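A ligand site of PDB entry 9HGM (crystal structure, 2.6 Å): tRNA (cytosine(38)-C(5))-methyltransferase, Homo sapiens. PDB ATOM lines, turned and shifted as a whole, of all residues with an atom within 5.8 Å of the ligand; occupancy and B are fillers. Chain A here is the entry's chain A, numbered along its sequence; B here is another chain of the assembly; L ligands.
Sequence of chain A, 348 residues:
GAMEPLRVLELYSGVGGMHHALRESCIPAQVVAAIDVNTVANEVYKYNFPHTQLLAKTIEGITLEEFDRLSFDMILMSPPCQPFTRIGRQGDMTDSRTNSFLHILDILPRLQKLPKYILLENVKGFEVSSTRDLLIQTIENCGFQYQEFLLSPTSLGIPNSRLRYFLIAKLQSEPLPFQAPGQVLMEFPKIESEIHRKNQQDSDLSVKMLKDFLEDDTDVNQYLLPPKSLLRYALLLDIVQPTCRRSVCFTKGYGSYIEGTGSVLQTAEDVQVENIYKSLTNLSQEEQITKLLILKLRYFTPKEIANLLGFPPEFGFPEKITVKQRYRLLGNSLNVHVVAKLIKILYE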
ATOM      1  N   TYR A  12      27.371   4.111 -15.977  1.00  0.00           N
ATOM      2  CA  TYR A  12      26.560   4.864 -15.018  1.00  0.00           C
ATOM      3  C   TYR A  12      27.293   5.008 -13.685  1.00  0.00           C
ATOM      4  O   TYR A  12      26.799   4.629 -12.617  1.00  0.00           O
ATOM      5  CB  TYR A  12      25.186   4.215 -14.839  1.00  0.00           C
ATOM      6  CG  TYR A  12      24.333   4.281 -16.073  1.00  0.00           C
ATOM      7  CD1 TYR A  12      23.984   5.502 -16.638  1.00  0.00           C
ATOM      8  CD2 TYR A  12      23.865   3.120 -16.679  1.00  0.00           C
ATOM      9  CE1 TYR A  12      23.187   5.563 -17.772  1.00  0.00           C
ATOM     10  CE2 TYR A  12      23.068   3.180 -17.813  1.00  0.00           C
ATOM     11  CZ  TYR A  12      22.735   4.397 -18.356  1.00  0.00           C
ATOM     12  OH  TYR A  12      21.961   4.454 -19.488  1.00  0.00           O
ATOM     13  N   MET A  77      28.086  -2.170 -13.893  1.00  0.00           N
ATOM     14  CA  MET A  77      27.020  -1.217 -14.150  1.00  0.00           C
ATOM     15  C   MET A  77      26.052  -1.163 -12.981  1.00  0.00           C
ATOM     16  O   MET A  77      25.696  -2.188 -12.410  1.00  0.00           O
ATOM     17  CB  MET A  77      26.267  -1.512 -15.425  1.00  0.00           C
ATOM     18  CG  MET A  77      25.313  -0.403 -15.830  1.00  0.00           C
ATOM     19  SD  MET A  77      24.669  -0.551 -17.507  1.00  0.00           S
ATOM     20  CE  MET A  77      23.809  -2.118 -17.381  1.00  0.00           C
ATOM     21  N   SER A  78      25.638   0.045 -12.641  1.00  0.00           N
ATOM     22  CA  SER A  78      24.766   0.369 -11.529  1.00  0.00           C
ATOM     23  C   SER A  78      23.671   1.292 -12.045  1.00  0.00           C
ATOM     24  O   SER A  78      23.874   2.028 -13.018  1.00  0.00           O
ATOM     25  CB  SER A  78      25.554   1.067 -10.402  1.00  0.00           C
ATOM     26  OG  SER A  78      24.778   1.202  -9.226  1.00  0.00           O
ATOM     27  N   PRO A  79      22.495   1.273 -11.426  1.00  0.00           N
ATOM     28  CA  PRO A  79      21.417   2.162 -11.866  1.00  0.00           C
ATOM     29  C   PRO A  79      21.889   3.609 -11.864  1.00  0.00           C
ATOM     30  O   PRO A  79      22.646   4.021 -10.977  1.00  0.00           O
ATOM     31  CB  PRO A  79      20.312   1.933 -10.808  1.00  0.00           C
ATOM     32  CG  PRO A  79      20.601   0.598 -10.263  1.00  0.00           C
ATOM     33  CD  PRO A  79      22.096   0.450 -10.275  1.00  0.00           C
ATOM     34  N   PRO A  80      21.464   4.401 -12.847  1.00  0.00           N
ATOM     35  CA  PRO A  80      21.708   5.850 -12.877  1.00  0.00           C
ATOM     36  C   PRO A  80      21.158   6.553 -11.638  1.00  0.00           C
ATOM     37  O   PRO A  80      20.167   6.085 -11.078  1.00  0.00           O
ATOM     38  CB  PRO A  80      20.962   6.309 -14.137  1.00  0.00           C
ATOM     39  CG  PRO A  80      20.006   5.213 -14.456  1.00  0.00           C
ATOM     40  CD  PRO A  80      20.675   3.959 -14.017  1.00  0.00           C
ATOM     41  N   GLN A  82      19.301   8.752 -11.149  1.00  0.00           N
ATOM     42  CA  GLN A  82      17.849   8.916 -11.286  1.00  0.00           C
ATOM     43  C   GLN A  82      17.268  10.100 -10.500  1.00  0.00           C
ATOM     44  O   GLN A  82      16.256   9.944  -9.834  1.00  0.00           O
ATOM     45  CB  GLN A  82      17.120   7.633 -10.858  1.00  0.00           C
ATOM     46  CG  GLN A  82      16.912   6.623 -11.973  1.00  0.00           C
ATOM     47  CD  GLN A  82      15.737   6.981 -12.884  1.00  0.00           C
ATOM     48  OE1 GLN A  82      15.148   8.067 -12.776  1.00  0.00           O
ATOM     49  NE2 GLN A  82      15.386   6.064 -13.797  1.00  0.00           N
ATOM     50  N   ARG A  97      18.337   6.012 -22.224  1.00  0.00           N
ATOM     51  CA  ARG A  97      18.390   4.724 -21.554  1.00  0.00           C
ATOM     52  C   ARG A  97      18.197   3.589 -22.542  1.00  0.00           C
ATOM     53  O   ARG A  97      19.008   2.651 -22.586  1.00  0.00           O
ATOM     54  CB  ARG A  97      17.332   4.660 -20.447  1.00  0.00           C
ATOM     55  CG  ARG A  97      17.516   5.640 -19.295  1.00  0.00           C
ATOM     56  CD  ARG A  97      16.697   5.172 -18.083  1.00  0.00           C
ATOM     57  NE  ARG A  97      16.279   6.260 -17.214  1.00  0.00           N
ATOM     58  CZ  ARG A  97      15.176   6.982 -17.394  1.00  0.00           C
ATOM     59  NH1 ARG A  97      14.383   6.795 -18.430  1.00  0.00           N
ATOM     60  NH2 ARG A  97      14.868   7.929 -16.513  1.00  0.00           N
ATOM     61  N   THR A  98      17.123   3.652 -23.348  1.00  0.00           N
ATOM     62  CA  THR A  98      16.837   2.573 -24.291  1.00  0.00           C
ATOM     63  C   THR A  98      18.011   2.345 -25.241  1.00  0.00           C
ATOM     64  O   THR A  98      18.576   1.241 -25.293  1.00  0.00           O
ATOM     65  CB  THR A  98      15.558   2.890 -25.078  1.00  0.00           C
ATOM     66  OG1 THR A  98      14.461   3.007 -24.174  1.00  0.00           O
ATOM     67  CG2 THR A  98      15.285   1.789 -26.081  1.00  0.00           C
ATOM     68  N   PHE A 101      21.193   0.892 -23.500  1.00  0.00           N
ATOM     69  CA  PHE A 101      21.110  -0.529 -23.145  1.00  0.00           C
ATOM     70  C   PHE A 101      21.188  -1.400 -24.392  1.00  0.00           C
ATOM     71  O   PHE A 101      21.944  -2.372 -24.441  1.00  0.00           O
ATOM     72  CB  PHE A 101      19.822  -0.792 -22.372  1.00  0.00           C
ATOM     73  CG  PHE A 101      19.558  -2.239 -22.072  1.00  0.00           C
ATOM     74  CD1 PHE A 101      20.202  -2.870 -21.027  1.00  0.00           C
ATOM     75  CD2 PHE A 101      18.654  -2.970 -22.833  1.00  0.00           C
ATOM     76  CE1 PHE A 101      19.961  -4.189 -20.739  1.00  0.00           C
ATOM     77  CE2 PHE A 101      18.407  -4.300 -22.552  1.00  0.00           C
ATOM     78  CZ  PHE A 101      19.067  -4.913 -21.506  1.00  0.00           C
ATOM     79  N   LEU A 120      26.390  -6.688 -12.688  1.00  0.00           N
ATOM     80  CA  LEU A 120      25.370  -5.656 -12.783  1.00  0.00           C
ATOM     81  C   LEU A 120      24.578  -5.613 -11.477  1.00  0.00           C
ATOM     82  O   LEU A 120      24.340  -6.647 -10.859  1.00  0.00           O
ATOM     83  CB  LEU A 120      24.412  -5.918 -13.951  1.00  0.00           C
ATOM     84  CG  LEU A 120      25.059  -6.322 -15.276  1.00  0.00           C
ATOM     85  CD1 LEU A 120      23.993  -6.538 -16.347  1.00  0.00           C
ATOM     86  CD2 LEU A 120      26.059  -5.265 -15.720  1.00  0.00           C
ATOM     87  N   GLU A 121      24.178  -4.406 -11.077  1.00  0.00           N
ATOM     88  CA  GLU A 121      23.325  -4.195  -9.924  1.00  0.00           C
ATOM     89  C   GLU A 121      22.099  -3.426 -10.377  1.00  0.00           C
ATOM     90  O   GLU A 121      22.210  -2.460 -11.151  1.00  0.00           O
ATOM     91  CB  GLU A 121      24.075  -3.450  -8.822  1.00  0.00           C
ATOM     92  CG  GLU A 121      23.428  -3.503  -7.447  1.00  0.00           C
ATOM     93  CD  GLU A 121      22.541  -2.309  -7.174  1.00  0.00           C
ATOM     94  OE1 GLU A 121      22.331  -1.499  -8.102  1.00  0.00           O
ATOM     95  OE2 GLU A 121      22.046  -2.183  -6.021  1.00  0.00           O
ATOM     96  N   ASN A 122      20.917  -3.851  -9.938  1.00  0.00           N
ATOM     97  CA  ASN A 122      19.663  -3.198 -10.336  1.00  0.00           C
ATOM     98  C   ASN A 122      18.678  -3.339  -9.184  1.00  0.00           C
ATOM     99  O   ASN A 122      18.929  -4.018  -8.192  1.00  0.00           O
ATOM    100  CB  ASN A 122      19.120  -3.805 -11.631  1.00  0.00           C
ATOM    101  CG  ASN A 122      18.271  -2.824 -12.430  1.00  0.00           C
ATOM    102  OD1 ASN A 122      17.878  -1.777 -11.914  1.00  0.00           O
ATOM    103  ND2 ASN A 122      17.980  -3.172 -13.682  1.00  0.00           N
ATOM    104  N   VAL A 123      17.527  -2.645  -9.328  1.00  0.00           N
ATOM    105  CA  VAL A 123      16.508  -2.654  -8.288  1.00  0.00           C
ATOM    106  C   VAL A 123      15.765  -3.995  -8.278  1.00  0.00           C
ATOM    107  O   VAL A 123      15.683  -4.690  -9.309  1.00  0.00           O
ATOM    108  CB  VAL A 123      15.527  -1.488  -8.485  1.00  0.00           C
ATOM    109  CG1 VAL A 123      16.238  -0.165  -8.511  1.00  0.00           C
ATOM    110  CG2 VAL A 123      14.733  -1.697  -9.772  1.00  0.00           C
ATOM    111  N   LYS A 124      15.219  -4.358  -7.126  1.00  0.00           N
ATOM    112  CA  LYS A 124      14.403  -5.558  -7.074  1.00  0.00           C
ATOM    113  C   LYS A 124      13.207  -5.419  -8.005  1.00  0.00           C
ATOM    114  O   LYS A 124      12.696  -4.307  -8.236  1.00  0.00           O
ATOM    115  CB  LYS A 124      13.920  -5.836  -5.647  1.00  0.00           C
ATOM    116  CG  LYS A 124      13.067  -4.742  -5.052  1.00  0.00           C
ATOM    117  CD  LYS A 124      12.479  -5.195  -3.725  1.00  0.00           C
ATOM    118  CE  LYS A 124      11.861  -4.050  -2.921  1.00  0.00           C
ATOM    119  NZ  LYS A 124      11.109  -4.573  -1.733  1.00  0.00           N
ATOM    120  N   GLY A 125      12.748  -6.547  -8.531  1.00  0.00           N
ATOM    121  CA  GLY A 125      11.701  -6.588  -9.504  1.00  0.00           C
ATOM    122  C   GLY A 125      12.198  -6.777 -10.920  1.00  0.00           C
ATOM    123  O   GLY A 125      11.491  -7.358 -11.749  1.00  0.00           O
ATOM    124  N   PHE A 126      13.409  -6.310 -11.211  1.00  0.00           N
ATOM    125  CA  PHE A 126      13.978  -6.498 -12.545  1.00  0.00           C
ATOM    126  C   PHE A 126      14.008  -7.957 -12.966  1.00  0.00           C
ATOM    127  O   PHE A 126      13.872  -8.272 -14.151  1.00  0.00           O
ATOM    128  CB  PHE A 126      15.390  -5.907 -12.588  1.00  0.00           C
ATOM    129  CG  PHE A 126      16.118  -6.136 -13.876  1.00  0.00           C
ATOM    130  CD1 PHE A 126      15.752  -5.443 -15.031  1.00  0.00           C
ATOM    131  CD2 PHE A 126      17.166  -7.040 -13.947  1.00  0.00           C
ATOM    132  CE1 PHE A 126      16.426  -5.662 -16.226  1.00  0.00           C
ATOM    133  CE2 PHE A 126      17.846  -7.247 -15.135  1.00  0.00           C
ATOM    134  CZ  PHE A 126      17.474  -6.557 -16.268  1.00  0.00           C
ATOM    135  N   SER A 129      11.380  -9.112 -15.486  1.00  0.00           N
ATOM    136  CA  SER A 129      11.027  -8.200 -16.562  1.00  0.00           C
ATOM    137  C   SER A 129      11.349  -8.800 -17.926  1.00  0.00           C
ATOM    138  O   SER A 129      12.254  -9.621 -18.062  1.00  0.00           O
ATOM    139  CB  SER A 129      11.758  -6.866 -16.390  1.00  0.00           C
ATOM    140  OG  SER A 129      13.159  -7.032 -16.534  1.00  0.00           O
ATOM    141  N   THR A 131      12.807  -7.161 -20.015  1.00  0.00           N
ATOM    142  CA  THR A 131      14.142  -6.646 -20.294  1.00  0.00           C
ATOM    143  C   THR A 131      15.212  -7.636 -19.811  1.00  0.00           C
ATOM    144  O   THR A 131      16.152  -7.958 -20.557  1.00  0.00           O
ATOM    145  CB  THR A 131      14.331  -5.285 -19.630  1.00  0.00           C
ATOM    146  OG1 THR A 131      13.313  -4.398 -20.085  1.00  0.00           O
ATOM    147  CG2 THR A 131      15.676  -4.705 -19.997  1.00  0.00           C
ATOM    148  N   LEU A 135      18.250  -9.439 -21.846  1.00  0.00           N
ATOM    149  CA  LEU A 135      19.616  -9.352 -21.343  1.00  0.00           C
ATOM    150  C   LEU A 135      20.224 -10.729 -21.154  1.00  0.00           C
ATOM    151  O   LEU A 135      21.345 -10.998 -21.628  1.00  0.00           O
ATOM    152  CB  LEU A 135      19.640  -8.570 -20.029  1.00  0.00           C
ATOM    153  CG  LEU A 135      20.925  -8.667 -19.213  1.00  0.00           C
ATOM    154  CD1 LEU A 135      22.084  -7.986 -19.936  1.00  0.00           C
ATOM    155  CD2 LEU A 135      20.717  -8.059 -17.839  1.00  0.00           C
ATOM    156  N   TYR A 165      18.895  -6.216  -6.875  1.00  0.00           N
ATOM    157  CA  TYR A 165      19.155  -7.280  -7.848  1.00  0.00           C
ATOM    158  C   TYR A 165      20.626  -7.254  -8.242  1.00  0.00           C
ATOM    159  O   TYR A 165      21.232  -6.170  -8.384  1.00  0.00           O
ATOM    160  CB  TYR A 165      18.268  -7.098  -9.074  1.00  0.00           C
ATOM    161  CG  TYR A 165      18.652  -7.923 -10.271  1.00  0.00           C
ATOM    162  CD1 TYR A 165      19.585  -7.453 -11.193  1.00  0.00           C
ATOM    163  CD2 TYR A 165      18.060  -9.170 -10.511  1.00  0.00           C
ATOM    164  CE1 TYR A 165      19.933  -8.206 -12.304  1.00  0.00           C
ATOM    165  CE2 TYR A 165      18.417  -9.925 -11.610  1.00  0.00           C
ATOM    166  CZ  TYR A 165      19.346  -9.434 -12.508  1.00  0.00           C
ATOM    167  OH  TYR A 165      19.700 -10.176 -13.611  1.00  0.00           O
ATOM    168  N   ASN A 332      19.304   6.113  -4.926  1.00  0.00           N
ATOM    169  CA  ASN A 332      19.291   4.952  -5.809  1.00  0.00           C
ATOM    170  C   ASN A 332      20.645   4.240  -5.846  1.00  0.00           C
ATOM    171  O   ASN A 332      20.877   3.426  -6.740  1.00  0.00           O
ATOM    172  CB  ASN A 332      18.870   5.375  -7.208  1.00  0.00           C
ATOM    173  CG  ASN A 332      18.288   4.211  -8.035  1.00  0.00           C
ATOM    174  OD1 ASN A 332      17.961   3.159  -7.500  1.00  0.00           O
ATOM    175  ND2 ASN A 332      18.166   4.423  -9.343  1.00  0.00           N
ATOM    176  N   LEU B 235      11.400   0.107 -21.961  1.00  0.00           N
ATOM    177  CA  LEU B 235      12.224  -0.967 -21.412  1.00  0.00           C
ATOM    178  C   LEU B 235      12.310  -0.930 -19.896  1.00  0.00           C
ATOM    179  O   LEU B 235      12.849  -1.885 -19.304  1.00  0.00           O
ATOM    180  CB  LEU B 235      13.610  -0.931 -22.026  1.00  0.00           C
ATOM    181  CG  LEU B 235      13.757  -1.669 -23.370  1.00  0.00           C
ATOM    182  CD1 LEU B 235      12.826  -1.091 -24.418  1.00  0.00           C
ATOM    183  CD2 LEU B 235      15.193  -1.646 -23.854  1.00  0.00           C
ATOM    184  N   LEU B 236      11.809   0.117 -19.243  1.00  0.00           N
ATOM    185  CA  LEU B 236      11.709   0.155 -17.790  1.00  0.00           C
ATOM    186  C   LEU B 236      10.349  -0.354 -17.298  1.00  0.00           C
ATOM    187  O   LEU B 236      10.113  -0.385 -16.074  1.00  0.00           O
ATOM    188  CB  LEU B 236      11.938   1.577 -17.271  1.00  0.00           C
ATOM    189  CG  LEU B 236      13.301   2.147 -17.583  1.00  0.00           C
ATOM    190  CD1 LEU B 236      13.336   3.623 -17.319  1.00  0.00           C
ATOM    191  CD2 LEU B 236      14.361   1.416 -16.776  1.00  0.00           C
ATOM    192  N   LEU B 237       9.461  -0.742 -18.201  1.00  0.00           N
ATOM    193  CA  LEU B 237       8.107  -1.143 -17.855  1.00  0.00           C
ATOM    194  C   LEU B 237       8.050  -2.610 -17.441  1.00  0.00           C
ATOM    195  O   LEU B 237       8.863  -3.435 -17.865  1.00  0.00           O
ATOM    196  CB  LEU B 237       7.165  -0.922 -19.042  1.00  0.00           C
ATOM    197  CG  LEU B 237       6.647   0.495 -19.275  1.00  0.00           C
ATOM    198  CD1 LEU B 237       5.978   0.568 -20.618  1.00  0.00           C
ATOM    199  CD2 LEU B 237       5.690   0.887 -18.157  1.00  0.00           C
ATOM    200  N   ASP B 238       7.069  -2.919 -16.604  1.00  0.00           N
ATOM    201  CA  ASP B 238       6.747  -4.313 -16.268  1.00  0.00           C
ATOM    202  C   ASP B 238       5.514  -4.698 -17.077  1.00  0.00           C
ATOM    203  O   ASP B 238       4.377  -4.446 -16.675  1.00  0.00           O
ATOM    204  CB  ASP B 238       6.510  -4.491 -14.778  1.00  0.00           C
ATOM    205  CG  ASP B 238       6.143  -5.927 -14.403  1.00  0.00           C
ATOM    206  OD1 ASP B 238       6.932  -6.850 -14.737  1.00  0.00           O
ATOM    207  OD2 ASP B 238       5.078  -6.133 -13.800  1.00  0.00           O
ATOM    208  N   GLU B 259       6.742   4.802 -13.222  1.00  0.00           N
ATOM    209  CA  GLU B 259       7.737   3.964 -12.562  1.00  0.00           C
ATOM    210  C   GLU B 259       7.325   3.682 -11.115  1.00  0.00           C
ATOM    211  O   GLU B 259       7.067   4.613 -10.343  1.00  0.00           O
ATOM    212  CB  GLU B 259       9.117   4.620 -12.593  1.00  0.00           C
ATOM    213  CG  GLU B 259       9.824   4.479 -13.925  1.00  0.00           C
ATOM    214  CD  GLU B 259      11.279   4.916 -13.832  1.00  0.00           C
ATOM    215  OE1 GLU B 259      11.538   6.122 -13.631  1.00  0.00           O
ATOM    216  OE2 GLU B 259      12.160   4.032 -13.939  1.00  0.00           O
HETATM  217  C1  LIG L   1      17.902   0.922 -18.203  1.00  0.00           C
HETATM  218  C2  LIG L   1      16.972   0.189 -19.158  1.00  0.00           C
HETATM  219  C3  LIG L   1      16.650  -1.305 -18.907  1.00  0.00           C
HETATM  220  C4  LIG L   1      15.696  -1.857 -16.606  1.00  0.00           C
HETATM  221  C5  LIG L   1      14.523  -2.304 -15.764  1.00  0.00           C
HETATM  222  C6  LIG L   1      14.441  -2.077 -14.394  1.00  0.00           C
HETATM  223  C7  LIG L   1      13.359  -2.524 -13.633  1.00  0.00           C
HETATM  224  C8  LIG L   1      12.308  -3.217 -14.204  1.00  0.00           C
HETATM  225  C9  LIG L   1      11.141  -3.699 -13.382  1.00  0.00           C
HETATM  226  C10 LIG L   1       9.906  -2.855 -13.423  1.00  0.00           C
HETATM  227  C11 LIG L   1      12.392  -3.457 -15.570  1.00  0.00           C
HETATM  228  C12 LIG L   1      13.451  -3.012 -16.323  1.00  0.00           C
HETATM  229  C13 LIG L   1      16.079   1.030 -20.074  1.00  0.00           C
HETATM  230  C14 LIG L   1      17.339   0.426 -20.628  1.00  0.00           C
HETATM  231  C15 LIG L   1      20.785   0.506 -16.270  1.00  0.00           C
HETATM  232  C16 LIG L   1      21.147  -0.762 -15.565  1.00  0.00           C
HETATM  233  C17 LIG L   1      21.904  -0.830 -14.406  1.00  0.00           C
HETATM  234  C18 LIG L   1      21.381  -2.975 -14.917  1.00  0.00           C
HETATM  235  C19 LIG L   1      21.258  -4.375 -14.898  1.00  0.00           C
HETATM  236  C20 LIG L   1      20.523  -4.951 -15.917  1.00  0.00           C
HETATM  237  C21 LIG L   1      14.197   3.862  -9.978  1.00  0.00           C
HETATM  238  C22 LIG L   1      15.550   2.328 -11.505  1.00  0.00           C
HETATM  239  C23 LIG L   1      15.469   1.279 -12.648  1.00  0.00           C
HETATM  240  C24 LIG L   1      17.508   1.446 -14.174  1.00  0.00           C
HETATM  241  C25 LIG L   1      18.822   0.794 -14.618  1.00  0.00           C
HETATM  242  C26 LIG L   1      19.312   1.046 -16.083  1.00  0.00           C
HETATM  243  C27 LIG L   1      19.935  -4.152 -16.909  1.00  0.00           C
HETATM  244  C28 LIG L   1      20.069  -2.767 -16.912  1.00  0.00           C
HETATM  245  C29 LIG L   1      20.801  -2.128 -15.901  1.00  0.00           C
HETATM  246  N1  LIG L   1      14.312   2.853 -11.056  1.00  0.00           N
HETATM  247  N2  LIG L   1      16.761   0.757 -13.169  1.00  0.00           N
HETATM  248  N3  LIG L   1      18.394   0.367 -17.016  1.00  0.00           N
HETATM  249  N4  LIG L   1      15.559  -1.657 -17.994  1.00  0.00           N
HETATM  250  N5  LIG L   1      22.043  -2.167 -14.002  1.00  0.00           N
HETATM  251  O1  LIG L   1      16.785  -1.714 -16.097  1.00  0.00           O
HETATM  252  O2  LIG L   1      18.256   2.047 -18.511  1.00  0.00           O
HETATM  253  O3  LIG L   1      17.099   2.473 -14.655  1.00  0.00           O
HETATM  254  O4  LIG L   1      16.598   2.707 -11.034  1.00  0.00           O
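ND2 of Asn 332 lies within hydrogen-bond range of O4 of the ligand (2.9 Å).
N4 of the ligand sits at hydrogen-bond distance from O of Leu 235 of chain B (3.0 Å).
The side-chain amide oxygen (OD1) of Asn 122 is in hydrogen-bond range of a nitrogen (N2) of the ligand (3.0 Å).
The backbone carbonyl oxygen (O) of Glu 121 sits at hydrogen-bond distance from a nitrogen (N5) of the ligand (2.9 Å).
The backbone carbonyl oxygen (O) of Phe 126 lies within hydrogen-bond range of the side-chain hydroxyl (OG) of Ser 129 (2.8 Å).
N of Glu 121 lies within hydrogen-bond range of O of Met 77 (3.0 Å).
The side-chain amide nitrogen (ND2) of Asn 332 sits at hydrogen-bond distance from the backbone carbonyl oxygen (O) of Pro 80 (3.1 Å).
O of Asn 122 sits at hydrogen-bond distance from N of Tyr 165 (2.6 Å).
The side-chain amide nitrogen (NE2) of Gln 82 lies close to the guanidinium group (NH2) of Arg 97, at 3.3 Å.
The backbone carbonyl oxygen (O) of Leu 235 of chain B lies within hydrogen-bond range of the side-chain hydroxyl (OG1) of Thr 131, 2.7 Å away.
Tyr 12 touches the ligand.
Met 77 touches the ligand.
C of Ser 78 touches C17 of the ligand, 3.6 Å away.
Pro 79 touches the ligand (N to C17, 3.7 Å).
Pro 80 touches the ligand (CD to C25, 3.7 Å).
Arg 97 touches the ligand (CB to O2, 3.4 Å).
Phe 101 touches the ligand.
CB of Leu 120 touches C19 of the ligand, at 3.6 Å.
Val 123 touches the ligand (CG1 to O4, 3.8 Å).
Phe 126 touches the ligand (CD1 to C5, 3.4 Å).
CB of Ser 129 touches C11 of the ligand, 3.6 Å away.
CG2 of Thr 131 touches N4 of the ligand (3.6 Å).
Leu 135 touches the ligand (CD2 to C20, 3.7 Å).
CD2 of Leu 236 of chain B touches N4 of the ligand, 3.5 Å away.
Glu 259 of chain B touches the ligand (OE2 to N1, 3.8 Å).
Hydrophobic or aromatic side chains that line the ligand: Tyr 12, Met 77, Pro 79, Pro 80, Phe 101, Leu 120, Val 123, Phe 126, Leu 135, Leu 235 of chain B and Leu 236 of chain B.
19 residues have an atom within 4 Å of the ligand: Tyr 12, Met 77, Ser 78, Pro 79, Pro 80, Arg 97, Phe 101, Leu 120, Glu 121, Asn 122, Val 123, Phe 126, Ser 129, Thr 131, Leu 135, Asn 332, Leu 235 of chain B, Leu 236 of chain B and Glu 259 of chain B.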
